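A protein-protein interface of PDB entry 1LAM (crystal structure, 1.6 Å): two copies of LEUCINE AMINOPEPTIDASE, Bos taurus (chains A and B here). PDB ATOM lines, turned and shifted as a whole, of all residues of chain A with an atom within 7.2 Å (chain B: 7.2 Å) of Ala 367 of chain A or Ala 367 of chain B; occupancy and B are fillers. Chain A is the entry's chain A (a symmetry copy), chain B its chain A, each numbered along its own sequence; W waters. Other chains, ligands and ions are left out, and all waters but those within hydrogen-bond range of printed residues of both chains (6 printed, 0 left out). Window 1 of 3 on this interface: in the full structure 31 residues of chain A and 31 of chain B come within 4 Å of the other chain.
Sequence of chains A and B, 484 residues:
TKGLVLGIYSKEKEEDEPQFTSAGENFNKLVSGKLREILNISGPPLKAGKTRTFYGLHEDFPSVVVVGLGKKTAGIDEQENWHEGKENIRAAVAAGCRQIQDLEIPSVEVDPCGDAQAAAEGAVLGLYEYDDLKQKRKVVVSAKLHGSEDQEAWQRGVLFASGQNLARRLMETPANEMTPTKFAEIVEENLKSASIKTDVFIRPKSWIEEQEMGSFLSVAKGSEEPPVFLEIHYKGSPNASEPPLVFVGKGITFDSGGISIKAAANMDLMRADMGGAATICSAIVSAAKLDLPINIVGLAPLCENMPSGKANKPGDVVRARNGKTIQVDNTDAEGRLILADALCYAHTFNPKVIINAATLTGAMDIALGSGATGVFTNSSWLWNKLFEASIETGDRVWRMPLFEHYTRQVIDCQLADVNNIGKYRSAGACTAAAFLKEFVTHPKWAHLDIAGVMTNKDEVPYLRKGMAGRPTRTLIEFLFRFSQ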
ATOM      1  N   GLY A 362     -36.692  -9.858 -12.664  1.00  0.00           N
ATOM      2  CA  GLY A 362     -36.026  -9.006 -13.634  1.00  0.00           C
ATOM      3  C   GLY A 362     -34.520  -9.093 -13.379  1.00  0.00           C
ATOM      4  O   GLY A 362     -33.717  -8.902 -14.286  1.00  0.00           O
ATOM      5  N   ALA A 363     -34.142  -9.395 -12.133  1.00  0.00           N
ATOM      6  CA  ALA A 363     -32.736  -9.541 -11.762  1.00  0.00           C
ATOM      7  C   ALA A 363     -32.068 -10.642 -12.599  1.00  0.00           C
ATOM      8  O   ALA A 363     -30.917 -10.495 -12.999  1.00  0.00           O
ATOM      9  CB  ALA A 363     -32.597  -9.846 -10.263  1.00  0.00           C
ATOM     10  N   MET A 364     -32.790 -11.726 -12.879  1.00  0.00           N
ATOM     11  CA  MET A 364     -32.220 -12.817 -13.671  1.00  0.00           C
ATOM     12  C   MET A 364     -31.879 -12.302 -15.063  1.00  0.00           C
ATOM     13  O   MET A 364     -30.832 -12.640 -15.626  1.00  0.00           O
ATOM     14  CB  MET A 364     -33.191 -14.007 -13.775  1.00  0.00           C
ATOM     15  CG  MET A 364     -32.575 -15.281 -14.385  1.00  0.00           C
ATOM     16  SD  MET A 364     -31.270 -15.962 -13.310  1.00  0.00           S
ATOM     17  CE  MET A 364     -29.955 -15.952 -14.378  1.00  0.00           C
ATOM     18  N   ASP A 365     -32.757 -11.461 -15.606  1.00  0.00           N
ATOM     19  CA  ASP A 365     -32.534 -10.882 -16.920  1.00  0.00           C
ATOM     20  C   ASP A 365     -31.274  -9.993 -16.869  1.00  0.00           C
ATOM     21  O   ASP A 365     -30.421 -10.049 -17.758  1.00  0.00           O
ATOM     22  CB  ASP A 365     -33.771 -10.077 -17.341  1.00  0.00           C
ATOM     23  CG  ASP A 365     -33.653  -9.523 -18.743  1.00  0.00           C
ATOM     24  OD1 ASP A 365     -34.046 -10.225 -19.684  1.00  0.00           O
ATOM     25  OD2 ASP A 365     -33.146  -8.391 -18.907  1.00  0.00           O
ATOM     26  N   ILE A 366     -31.152  -9.180 -15.821  1.00  0.00           N
ATOM     27  CA  ILE A 366     -29.974  -8.319 -15.684  1.00  0.00           C
ATOM     28  C   ILE A 366     -28.726  -9.189 -15.525  1.00  0.00           C
ATOM     29  O   ILE A 366     -27.657  -8.821 -15.994  1.00  0.00           O
ATOM     30  CB  ILE A 366     -30.078  -7.371 -14.452  1.00  0.00           C
ATOM     31  CG1 ILE A 366     -31.251  -6.406 -14.615  1.00  0.00           C
ATOM     32  CG2 ILE A 366     -28.784  -6.597 -14.248  1.00  0.00           C
ATOM     33  CD1 ILE A 366     -31.220  -5.594 -15.894  1.00  0.00           C
ATOM     34  N   ALA A 367     -28.876 -10.345 -14.877  1.00  0.00           N
ATOM     35  CA  ALA A 367     -27.757 -11.268 -14.630  1.00  0.00           C
ATOM     36  C   ALA A 367     -27.198 -12.006 -15.852  1.00  0.00           C
ATOM     37  O   ALA A 367     -26.001 -11.924 -16.128  1.00  0.00           O
ATOM     38  CB  ALA A 367     -28.139 -12.289 -13.523  1.00  0.00           C
ATOM     39  N   LEU A 368     -28.053 -12.714 -16.583  1.00  0.00           N
ATOM     40  CA  LEU A 368     -27.604 -13.501 -17.741  1.00  0.00           C
ATOM     41  C   LEU A 368     -28.316 -13.192 -19.053  1.00  0.00           C
ATOM     42  O   LEU A 368     -27.941 -13.730 -20.103  1.00  0.00           O
ATOM     43  CB  LEU A 368     -27.765 -15.001 -17.448  1.00  0.00           C
ATOM     44  CG  LEU A 368     -27.036 -15.589 -16.234  1.00  0.00           C
ATOM     45  CD1 LEU A 368     -27.295 -17.095 -16.153  1.00  0.00           C
ATOM     46  CD2 LEU A 368     -25.540 -15.304 -16.351  1.00  0.00           C
ATOM     47  N   GLY A 369     -29.331 -12.332 -19.009  1.00  0.00           N
ATOM     48  CA  GLY A 369     -30.060 -12.020 -20.225  1.00  0.00           C
ATOM     49  C   GLY A 369     -30.688 -13.272 -20.832  1.00  0.00           C
ATOM     50  O   GLY A 369     -31.236 -14.117 -20.112  1.00  0.00           O
ATOM     51  N   PHE A 376     -31.017 -22.918  -9.946  1.00  0.00           N
ATOM     52  CA  PHE A 376     -30.672 -22.961  -8.524  1.00  0.00           C
ATOM     53  C   PHE A 376     -31.013 -24.378  -8.065  1.00  0.00           C
ATOM     54  O   PHE A 376     -32.166 -24.799  -8.170  1.00  0.00           O
ATOM     55  CB  PHE A 376     -31.521 -21.957  -7.735  1.00  0.00           C
ATOM     56  CG  PHE A 376     -31.225 -20.512  -8.056  1.00  0.00           C
ATOM     57  CD1 PHE A 376     -31.892 -19.855  -9.090  1.00  0.00           C
ATOM     58  CD2 PHE A 376     -30.299 -19.795  -7.297  1.00  0.00           C
ATOM     59  CE1 PHE A 376     -31.655 -18.500  -9.369  1.00  0.00           C
ATOM     60  CE2 PHE A 376     -30.052 -18.431  -7.565  1.00  0.00           C
ATOM     61  CZ  PHE A 376     -30.737 -17.787  -8.608  1.00  0.00           C
ATOM     62  N   MET A 400     -26.734 -20.995 -10.642  1.00  0.00           N
ATOM     63  CA  MET A 400     -26.737 -19.795  -9.797  1.00  0.00           C
ATOM     64  C   MET A 400     -26.713 -20.325  -8.357  1.00  0.00           C
ATOM     65  O   MET A 400     -27.254 -21.405  -8.077  1.00  0.00           O
ATOM     66  CB  MET A 400     -27.955 -18.921 -10.088  1.00  0.00           C
ATOM     67  CG  MET A 400     -27.947 -18.324 -11.488  1.00  0.00           C
ATOM     68  SD  MET A 400     -26.653 -17.082 -11.718  1.00  0.00           S
ATOM     69  CE  MET A 400     -27.457 -15.639 -11.013  1.00  0.00           C
ATOM     70  N   PRO A 401     -26.140 -19.555  -7.416  1.00  0.00           N
ATOM     71  CA  PRO A 401     -26.038 -20.009  -6.022  1.00  0.00           C
ATOM     72  C   PRO A 401     -27.221 -20.083  -5.054  1.00  0.00           C
ATOM     73  O   PRO A 401     -28.041 -19.161  -4.973  1.00  0.00           O
ATOM     74  CB  PRO A 401     -24.931 -19.112  -5.471  1.00  0.00           C
ATOM     75  CG  PRO A 401     -25.215 -17.799  -6.145  1.00  0.00           C
ATOM     76  CD  PRO A 401     -25.589 -18.193  -7.576  1.00  0.00           C
ATOM     77  N   TYR A 406     -28.088 -15.641   1.218  1.00  0.00           N
ATOM     78  CA  TYR A 406     -29.290 -15.062   0.625  1.00  0.00           C
ATOM     79  C   TYR A 406     -30.522 -15.330   1.486  1.00  0.00           C
ATOM     80  O   TYR A 406     -31.385 -14.456   1.643  1.00  0.00           O
ATOM     81  CB  TYR A 406     -29.481 -15.583  -0.806  1.00  0.00           C
ATOM     82  CG  TYR A 406     -28.283 -15.308  -1.692  1.00  0.00           C
ATOM     83  CD1 TYR A 406     -27.888 -13.993  -1.979  1.00  0.00           C
ATOM     84  CD2 TYR A 406     -27.515 -16.351  -2.206  1.00  0.00           C
ATOM     85  CE1 TYR A 406     -26.759 -13.731  -2.752  1.00  0.00           C
ATOM     86  CE2 TYR A 406     -26.382 -16.105  -2.977  1.00  0.00           C
ATOM     87  CZ  TYR A 406     -26.005 -14.794  -3.250  1.00  0.00           C
ATOM     88  OH  TYR A 406     -24.877 -14.543  -4.010  1.00  0.00           O
ATOM     89  N   ARG A 425     -31.468  -4.565  -2.459  1.00  0.00           N
ATOM     90  CA  ARG A 425     -31.841  -4.713  -3.864  1.00  0.00           C
ATOM     91  C   ARG A 425     -30.908  -5.654  -4.636  1.00  0.00           C
ATOM     92  O   ARG A 425     -31.204  -6.053  -5.753  1.00  0.00           O
ATOM     93  CB  ARG A 425     -31.838  -3.343  -4.543  1.00  0.00           C
ATOM     94  CG  ARG A 425     -32.634  -2.267  -3.800  1.00  0.00           C
ATOM     95  CD  ARG A 425     -31.843  -0.966  -3.758  1.00  0.00           C
ATOM     96  NE  ARG A 425     -32.581   0.184  -4.287  1.00  0.00           N
ATOM     97  CZ  ARG A 425     -32.974   0.329  -5.555  1.00  0.00           C
ATOM     98  NH1 ARG A 425     -32.724  -0.613  -6.467  1.00  0.00           N
ATOM     99  NH2 ARG A 425     -33.636   1.427  -5.914  1.00  0.00           N
ATOM    100  N   SER A 426     -29.776  -5.990  -4.035  1.00  0.00           N
ATOM    101  CA  SER A 426     -28.795  -6.852  -4.674  1.00  0.00           C
ATOM    102  C   SER A 426     -29.231  -8.316  -4.797  1.00  0.00           C
ATOM    103  O   SER A 426     -30.030  -8.789  -4.001  1.00  0.00           O
ATOM    104  CB  SER A 426     -27.507  -6.793  -3.862  1.00  0.00           C
ATOM    105  OG  SER A 426     -27.131  -5.446  -3.639  1.00  0.00           O
ATOM    106  N   ALA A 427     -28.698  -9.015  -5.797  1.00  0.00           N
ATOM    107  CA  ALA A 427     -28.966 -10.448  -5.981  1.00  0.00           C
ATOM    108  C   ALA A 427     -30.431 -10.869  -5.937  1.00  0.00           C
ATOM    109  O   ALA A 427     -30.744 -11.904  -5.363  1.00  0.00           O
ATOM    110  CB  ALA A 427     -28.167 -11.251  -4.947  1.00  0.00           C
ATOM    111  N   GLY A 428     -31.300 -10.124  -6.615  1.00  0.00           N
ATOM    112  CA  GLY A 428     -32.727 -10.418  -6.619  1.00  0.00           C
ATOM    113  C   GLY A 428     -33.132 -11.832  -7.003  1.00  0.00           C
ATOM    114  O   GLY A 428     -34.074 -12.380  -6.435  1.00  0.00           O
ATOM    115  N   ALA A 429     -32.444 -12.423  -7.974  1.00  0.00           N
ATOM    116  CA  ALA A 429     -32.764 -13.796  -8.379  1.00  0.00           C
ATOM    117  C   ALA A 429     -32.361 -14.795  -7.286  1.00  0.00           C
ATOM    118  O   ALA A 429     -33.040 -15.812  -7.082  1.00  0.00           O
ATOM    119  CB  ALA A 429     -32.074 -14.151  -9.691  1.00  0.00           C
ATOM    120  N   CYS A 430     -31.257 -14.500  -6.594  1.00  0.00           N
ATOM    121  CA  CYS A 430     -30.736 -15.355  -5.530  1.00  0.00           C
ATOM    122  C   CYS A 430     -31.610 -15.326  -4.265  1.00  0.00           C
ATOM    123  O   CYS A 430     -31.851 -16.379  -3.644  1.00  0.00           O
ATOM    124  CB  CYS A 430     -29.285 -14.985  -5.210  1.00  0.00           C
ATOM    125  SG  CYS A 430     -28.137 -15.144  -6.595  1.00  0.00           S
ATOM    126  N   THR A 431     -32.078 -14.142  -3.870  1.00  0.00           N
ATOM    127  CA  THR A 431     -32.954 -14.058  -2.697  1.00  0.00           C
ATOM    128  C   THR A 431     -34.332 -14.662  -3.030  1.00  0.00           C
ATOM    129  O   THR A 431     -34.963 -15.263  -2.169  1.00  0.00           O
ATOM    130  CB  THR A 431     -33.106 -12.600  -2.194  1.00  0.00           C
ATOM    131  OG1 THR A 431     -33.458 -11.744  -3.290  1.00  0.00           O
ATOM    132  CG2 THR A 431     -31.800 -12.123  -1.553  1.00  0.00           C
ATOM    133  N   GLY B 362     -22.691  -2.601 -12.197  1.00  0.00           N
ATOM    134  CA  GLY B 362     -23.771  -2.656 -11.227  1.00  0.00           C
ATOM    135  C   GLY B 362     -24.568  -3.936 -11.482  1.00  0.00           C
ATOM    136  O   GLY B 362     -25.187  -4.483 -10.576  1.00  0.00           O
ATOM    137  N   ALA B 363     -24.540  -4.417 -12.729  1.00  0.00           N
ATOM    138  CA  ALA B 363     -25.231  -5.650 -13.101  1.00  0.00           C
ATOM    139  C   ALA B 363     -24.716  -6.832 -12.266  1.00  0.00           C
ATOM    140  O   ALA B 363     -25.500  -7.688 -11.867  1.00  0.00           O
ATOM    141  CB  ALA B 363     -25.063  -5.937 -14.600  1.00  0.00           C
ATOM    142  N   MET B 364     -23.414  -6.867 -11.987  1.00  0.00           N
ATOM    143  CA  MET B 364     -22.850  -7.963 -11.197  1.00  0.00           C
ATOM    144  C   MET B 364     -23.467  -7.946  -9.805  1.00  0.00           C
ATOM    145  O   MET B 364     -23.794  -8.997  -9.242  1.00  0.00           O
ATOM    146  CB  MET B 364     -21.319  -7.855 -11.094  1.00  0.00           C
ATOM    147  CG  MET B 364     -20.632  -9.093 -10.486  1.00  0.00           C
ATOM    148  SD  MET B 364     -20.828 -10.551 -11.563  1.00  0.00           S
ATOM    149  CE  MET B 364     -21.594 -11.621 -10.496  1.00  0.00           C
ATOM    150  N   ASP B 365     -23.648  -6.745  -9.260  1.00  0.00           N
ATOM    151  CA  ASP B 365     -24.249  -6.594  -7.945  1.00  0.00           C
ATOM    152  C   ASP B 365     -25.701  -7.111  -7.996  1.00  0.00           C
ATOM    153  O   ASP B 365     -26.147  -7.842  -7.108  1.00  0.00           O
ATOM    154  CB  ASP B 365     -24.193  -5.121  -7.522  1.00  0.00           C
ATOM    155  CG  ASP B 365     -24.713  -4.900  -6.120  1.00  0.00           C
ATOM    156  OD1 ASP B 365     -23.912  -4.985  -5.179  1.00  0.00           O
ATOM    157  OD2 ASP B 365     -25.929  -4.661  -5.954  1.00  0.00           O
ATOM    158  N   ILE B 366     -26.437  -6.742  -9.043  1.00  0.00           N
ATOM    159  CA  ILE B 366     -27.820  -7.208  -9.180  1.00  0.00           C
ATOM    160  C   ILE B 366     -27.828  -8.729  -9.341  1.00  0.00           C
ATOM    161  O   ILE B 366     -28.744  -9.391  -8.871  1.00  0.00           O
ATOM    162  CB  ILE B 366     -28.535  -6.575 -10.410  1.00  0.00           C
ATOM    163  CG1 ILE B 366     -28.647  -5.061 -10.245  1.00  0.00           C
ATOM    164  CG2 ILE B 366     -29.914  -7.186 -10.613  1.00  0.00           C
ATOM    165  CD1 ILE B 366     -29.328  -4.619  -8.965  1.00  0.00           C
ATOM    166  N   ALA B 367     -26.797  -9.272  -9.990  1.00  0.00           N
ATOM    167  CA  ALA B 367     -26.688 -10.718 -10.239  1.00  0.00           C
ATOM    168  C   ALA B 367     -26.407 -11.601  -9.019  1.00  0.00           C
ATOM    169  O   ALA B 367     -27.163 -12.533  -8.743  1.00  0.00           O
ATOM    170  CB  ALA B 367     -25.635 -10.993 -11.347  1.00  0.00           C
ATOM    171  N   LEU B 368     -25.334 -11.312  -8.288  1.00  0.00           N
ATOM    172  CA  LEU B 368     -24.950 -12.134  -7.131  1.00  0.00           C
ATOM    173  C   LEU B 368     -24.791 -11.376  -5.819  1.00  0.00           C
ATOM    174  O   LEU B 368     -24.566 -11.994  -4.770  1.00  0.00           O
ATOM    175  CB  LEU B 368     -23.631 -12.867  -7.426  1.00  0.00           C
ATOM    176  CG  LEU B 368     -23.572 -13.799  -8.641  1.00  0.00           C
ATOM    177  CD1 LEU B 368     -22.192 -14.456  -8.724  1.00  0.00           C
ATOM    178  CD2 LEU B 368     -24.667 -14.858  -8.525  1.00  0.00           C
ATOM    179  N   GLY B 369     -24.909 -10.050  -5.860  1.00  0.00           N
ATOM    180  CA  GLY B 369     -24.742  -9.277  -4.643  1.00  0.00           C
ATOM    181  C   GLY B 369     -23.357  -9.486  -4.038  1.00  0.00           C
ATOM    182  O   GLY B 369     -22.351  -9.524  -4.758  1.00  0.00           O
ATOM    183  N   PHE B 376     -15.293 -14.763 -14.936  1.00  0.00           N
ATOM    184  CA  PHE B 376     -15.457 -15.067 -16.359  1.00  0.00           C
ATOM    185  C   PHE B 376     -14.102 -15.605 -16.819  1.00  0.00           C
ATOM    186  O   PHE B 376     -13.094 -14.906 -16.714  1.00  0.00           O
ATOM    187  CB  PHE B 376     -15.789 -13.794 -17.146  1.00  0.00           C
ATOM    188  CG  PHE B 376     -17.140 -13.204 -16.823  1.00  0.00           C
ATOM    189  CD1 PHE B 376     -17.292 -12.280 -15.787  1.00  0.00           C
ATOM    190  CD2 PHE B 376     -18.260 -13.546 -17.582  1.00  0.00           C
ATOM    191  CE1 PHE B 376     -18.535 -11.694 -15.507  1.00  0.00           C
ATOM    192  CE2 PHE B 376     -19.517 -12.962 -17.312  1.00  0.00           C
ATOM    193  CZ  PHE B 376     -19.647 -12.032 -16.267  1.00  0.00           C
ATOM    194  N   MET B 400     -19.332 -17.154 -14.241  1.00  0.00           N
ATOM    195  CA  MET B 400     -20.312 -16.460 -15.084  1.00  0.00           C
ATOM    196  C   MET B 400     -19.893 -16.782 -16.525  1.00  0.00           C
ATOM    197  O   MET B 400     -18.699 -16.963 -16.806  1.00  0.00           O
ATOM    198  CB  MET B 400     -20.323 -14.961 -14.791  1.00  0.00           C
ATOM    199  CG  MET B 400     -20.815 -14.625 -13.390  1.00  0.00           C
ATOM    200  SD  MET B 400     -22.575 -14.968 -13.159  1.00  0.00           S
ATOM    201  CE  MET B 400     -23.292 -13.478 -13.862  1.00  0.00           C
ATOM    202  N   PRO B 401     -20.853 -16.806 -17.465  1.00  0.00           N
ATOM    203  CA  PRO B 401     -20.542 -17.149 -18.860  1.00  0.00           C
ATOM    204  C   PRO B 401     -19.801 -16.224 -19.827  1.00  0.00           C
ATOM    205  O   PRO B 401     -20.081 -15.023 -19.907  1.00  0.00           O
ATOM    206  CB  PRO B 401     -21.914 -17.537 -19.411  1.00  0.00           C
ATOM    207  CG  PRO B 401     -22.822 -16.548 -18.735  1.00  0.00           C
ATOM    208  CD  PRO B 401     -22.284 -16.472 -17.304  1.00  0.00           C
ATOM    209  N   TYR B 406     -22.935 -12.946 -26.092  1.00  0.00           N
ATOM    210  CA  TYR B 406     -22.715 -11.631 -25.498  1.00  0.00           C
ATOM    211  C   TYR B 406     -21.786 -10.778 -26.358  1.00  0.00           C
ATOM    212  O   TYR B 406     -22.003  -9.569 -26.514  1.00  0.00           O
ATOM    213  CB  TYR B 406     -22.178 -11.778 -24.067  1.00  0.00           C
ATOM    214  CG  TYR B 406     -23.093 -12.600 -23.182  1.00  0.00           C
ATOM    215  CD1 TYR B 406     -24.395 -12.164 -22.894  1.00  0.00           C
ATOM    216  CD2 TYR B 406     -22.682 -13.829 -22.670  1.00  0.00           C
ATOM    217  CE1 TYR B 406     -25.259 -12.937 -22.121  1.00  0.00           C
ATOM    218  CE2 TYR B 406     -23.537 -14.614 -21.900  1.00  0.00           C
ATOM    219  CZ  TYR B 406     -24.825 -14.167 -21.625  1.00  0.00           C
ATOM    220  OH  TYR B 406     -25.679 -14.944 -20.865  1.00  0.00           O
ATOM    221  N   ARG B 425     -30.035  -3.805 -22.398  1.00  0.00           N
ATOM    222  CA  ARG B 425     -29.698  -3.588 -20.994  1.00  0.00           C
ATOM    223  C   ARG B 425     -29.467  -4.894 -20.223  1.00  0.00           C
ATOM    224  O   ARG B 425     -28.969  -4.883 -19.106  1.00  0.00           O
ATOM    225  CB  ARG B 425     -30.819  -2.801 -20.313  1.00  0.00           C
ATOM    226  CG  ARG B 425     -31.240  -1.530 -21.054  1.00  0.00           C
ATOM    227  CD  ARG B 425     -32.759  -1.426 -21.094  1.00  0.00           C
ATOM    228  NE  ARG B 425     -33.272  -0.161 -20.564  1.00  0.00           N
ATOM    229  CZ  ARG B 425     -33.164   0.243 -19.294  1.00  0.00           C
ATOM    230  NH1 ARG B 425     -32.538  -0.506 -18.385  1.00  0.00           N
ATOM    231  NH2 ARG B 425     -33.679   1.416 -18.933  1.00  0.00           N
ATOM    232  N   SER B 426     -29.845  -6.011 -20.825  1.00  0.00           N
ATOM    233  CA  SER B 426     -29.705  -7.311 -20.188  1.00  0.00           C
ATOM    234  C   SER B 426     -28.258  -7.798 -20.067  1.00  0.00           C
ATOM    235  O   SER B 426     -27.411  -7.417 -20.863  1.00  0.00           O
ATOM    236  CB  SER B 426     -30.497  -8.328 -21.001  1.00  0.00           C
ATOM    237  OG  SER B 426     -31.814  -7.859 -21.223  1.00  0.00           O
ATOM    238  N   ALA B 427     -27.993  -8.638 -19.069  1.00  0.00           N
ATOM    239  CA  ALA B 427     -26.667  -9.245 -18.886  1.00  0.00           C
ATOM    240  C   ALA B 427     -25.479  -8.291 -18.930  1.00  0.00           C
ATOM    241  O   ALA B 427     -24.453  -8.631 -19.505  1.00  0.00           O
ATOM    242  CB  ALA B 427     -26.473 -10.360 -19.922  1.00  0.00           C
ATOM    243  N   GLY B 428     -25.587  -7.153 -18.250  1.00  0.00           N
ATOM    244  CA  GLY B 428     -24.524  -6.156 -18.245  1.00  0.00           C
ATOM    245  C   GLY B 428     -23.135  -6.640 -17.863  1.00  0.00           C
ATOM    246  O   GLY B 428     -22.144  -6.186 -18.432  1.00  0.00           O
ATOM    247  N   ALA B 429     -23.047  -7.544 -16.893  1.00  0.00           N
ATOM    248  CA  ALA B 429     -21.741  -8.075 -16.490  1.00  0.00           C
ATOM    249  C   ALA B 429     -21.157  -8.978 -17.585  1.00  0.00           C
ATOM    250  O   ALA B 429     -19.936  -9.010 -17.790  1.00  0.00           O
ATOM    251  CB  ALA B 429     -21.847  -8.845 -15.179  1.00  0.00           C
ATOM    252  N   CYS B 430     -22.035  -9.710 -18.277  1.00  0.00           N
ATOM    253  CA  CYS B 430     -21.637 -10.627 -19.343  1.00  0.00           C
ATOM    254  C   CYS B 430     -21.158  -9.894 -20.607  1.00  0.00           C
ATOM    255  O   CYS B 430     -20.160 -10.304 -21.229  1.00  0.00           O
ATOM    256  CB  CYS B 430     -22.776 -11.599 -19.663  1.00  0.00           C
ATOM    257  SG  CYS B 430     -23.307 -12.630 -18.279  1.00  0.00           S
ATOM    258  N   THR B 431     -21.856  -8.829 -21.000  1.00  0.00           N
ATOM    259  CA  THR B 431     -21.421  -8.063 -22.172  1.00  0.00           C
ATOM    260  C   THR B 431     -20.133  -7.286 -21.839  1.00  0.00           C
ATOM    261  O   THR B 431     -19.278  -7.115 -22.701  1.00  0.00           O
ATOM    262  CB  THR B 431     -22.525  -7.097 -22.673  1.00  0.00           C
ATOM    263  OG1 THR B 431     -23.021  -6.318 -21.575  1.00  0.00           O
ATOM    264  CG2 THR B 431     -23.668  -7.889 -23.314  1.00  0.00           C
HETATM  265  O   HOH W   1     -24.997  -9.331 -15.696  1.00  0.00           O
HETATM  266  O   HOH W   2     -23.869  -6.157  -2.851  1.00  0.00           O
HETATM  267  O   HOH W   3     -25.280  -2.755  -3.287  1.00  0.00           O
HETATM  268  O   HOH W   4     -29.862 -11.858  -9.172  1.00  0.00           O
HETATM  269  O   HOH W   5     -33.113 -10.933 -22.014  1.00  0.00           O
HETATM  270  O   HOH W   6     -35.081  -7.819 -21.573  1.00  0.00           O
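Water W2 bridges the side-chain carboxylate of Asp 365 of chain B (2.6 Å) and the side-chain hydroxyl of Ser 426 of chain A (3.4 Å).
Water W5 lies within hydrogen-bond range of the side-chain carboxylate of Asp 365 of chain A (2.6 Å) and the side-chain hydroxyl of Ser 426 of chain B (3.4 Å).
Among the printed residues, pairs that only touch across the chains: Leu 368 of chain A with Ala 427 of chain B (3.5 Å), Ala 427 of chain A with Leu 368 of chain B (3.5 Å), Ala 367 of chain A with Ala 367 of chain B (3.6 Å), Pro 401 of chain A with Leu 368 of chain B (3.6 Å), Leu 368 of chain A with Pro 401 of chain B (3.6 Å), Gly 369 of chain A with Ala 427 of chain B (3.6 Å), Ala 427 of chain A with Gly 369 of chain B (3.6 Å), Ala 363 of chain A with Ile 366 of chain B (3.8 Å), Ile 366 of chain A with Ala 363 of chain B (3.8 Å), Gly 369 of chain A with Ser 426 of chain B (3.8 Å), Ser 426 of chain A with Gly 369 of chain B (3.8 Å), Leu 368 of chain A with Met 400 of chain B (3.8 Å), Met 400 of chain A with Leu 368 of chain B (3.8 Å), Ile 366 of chain A with Ile 366 of chain B (3.8 Å), Met 400 of chain A with Ala 367 of chain B (3.9 Å), Ala 367 of chain A with Met 400 of chain B (3.9 Å), Ala 427 of chain A with Ala 367 of chain B (3.9 Å), Ala 367 of chain A with Ala 427 of chain B (3.9 Å), Cys 430 of chain A with Leu 368 of chain B (3.98 Å), Leu 368 of chain A with Cys 430 of chain B (3.98 Å), Ile 366 of chain A with Arg 425 of chain B (3.99 Å) and Arg 425 of chain A with Ile 366 of chain B (3.99 Å).
Ala 367 of chain A touches just these residues of chain B: Ala 367, Met 400, Ala 427 and Cys 430.
Ala 367 of chain B touches four residues of chain A.
Of the printed residues of chain B, Cys 430 of chain A touches Ala 367 (3.5 Å) and Leu 368 (3.98 Å).
Of the printed residues of chain B, Arg 425 of chain A touches Ile 366.
Printed residues of chain A within 4 Å of Ser 426 of chain B: Asp 365 and Gly 369.
Printed residues of chain A within 4 Å of Gly 428 of chain B: Ile 366.
The nearest residue of chain A that does not touch Ala 367 of chain B is Ala 363 of chain A (5.1 Å).
The nearest printed residue of chain A that does not touch Ala 363 of chain B is Ala 367 of chain A (5.1 Å).
The side-chain hydroxyl (OG) of Ser 426 of chain A is in hydrogen-bond range of the side-chain carboxylate (OD2) of Asp 365 of chain B.
The backbone carbonyl oxygen (O) of Asp 365 of chain B is in hydrogen-bond range of the backbone NH (N) of Ala 427 of chain A, at 3.1 Å.
The backbone NH (N) of Ala 427 of chain A lies close to the backbone carbonyl oxygen (O) of Ile 366 of chain B (3.1 Å).
The backbone carbonyl oxygen (O) of Ile 366 of chain B sits at hydrogen-bond distance from the backbone NH (N) of Gly 428 of chain A (3.5 Å).
The backbone carbonyl oxygen (O) of Ala 367 of chain B sits at hydrogen-bond distance from the side-chain sulfur (SG) of Cys 430 of chain A (3.5 Å).
The backbone carbonyl oxygen of Leu 368 of chain B lies within hydrogen-bond range of the side-chain hydroxyl of Tyr 406 of chain A, 2.7 Å away.
OH of Tyr 406 of chain B sits at hydrogen-bond distance from O of Leu 368 of chain A.
OG of Ser 426 of chain B lies within hydrogen-bond range of OD2 of Asp 365 of chain A, at 2.7 Å.
N of Ala 427 of chain B sits at hydrogen-bond distance from O of Asp 365 of chain A, at 3.1 Å.
N of Ala 427 of chain B sits close to O of Ile 366 of chain A, at 3.1 Å.
The backbone carbonyl oxygen (O) of Ile 366 of chain A is in hydrogen-bond range of the backbone NH (N) of Gly 428 of chain B.
SG of Cys 430 of chain B is in hydrogen-bond range of O of Ala 367 of chain A (3.5 Å).
Of the 19 printed residues of chain A, 14 touch a printed residue of chain B.
Along chain A the printed residues that touch a printed residue of chain B span positions 363 to 430.
Of the 19 printed residues of chain B, 14 touch a printed residue of chain A.
Hydrophobic or aromatic side chains of chain B that line the printed part of chain A: Ala 363, Ile 366, Ala 367, Leu 368, Met 400, Pro 401, Tyr 406 and Ala 427.
Among the printed residues, 34 pairs touch across the chains.
Among the printed residues, no Asp or Glu carboxylate lies within 4 Å of a Lys or Arg side-chain nitrogen of the other chain.
The side-chain hydroxyl of Thr 431 of chain B sits at hydrogen-bond distance from the backbone carbonyl oxygen of Ala 427 of chain B, 3.4 Å away.
The backbone carbonyl oxygen (O) of Ala 427 of chain A sits at hydrogen-bond distance from the side-chain hydroxyl (OG1) of Thr 431 of chain A.
O of Gly 428 of chain A lies within hydrogen-bond range of OG1 of Thr 431 of chain A (3.3 Å).
Asp 365 of chain A touches Ala 427 of chain B, and with the chains exchanged Ala 427 of chain A touches Asp 365 of chain B.
Ile 366 of chain B touches its own counterpart, Ile 366 of chain A.
Ile 366 of chain A touches Gly 428 of chain B, and with the chains exchanged Gly 428 of chain A touches Ile 366 of chain B.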
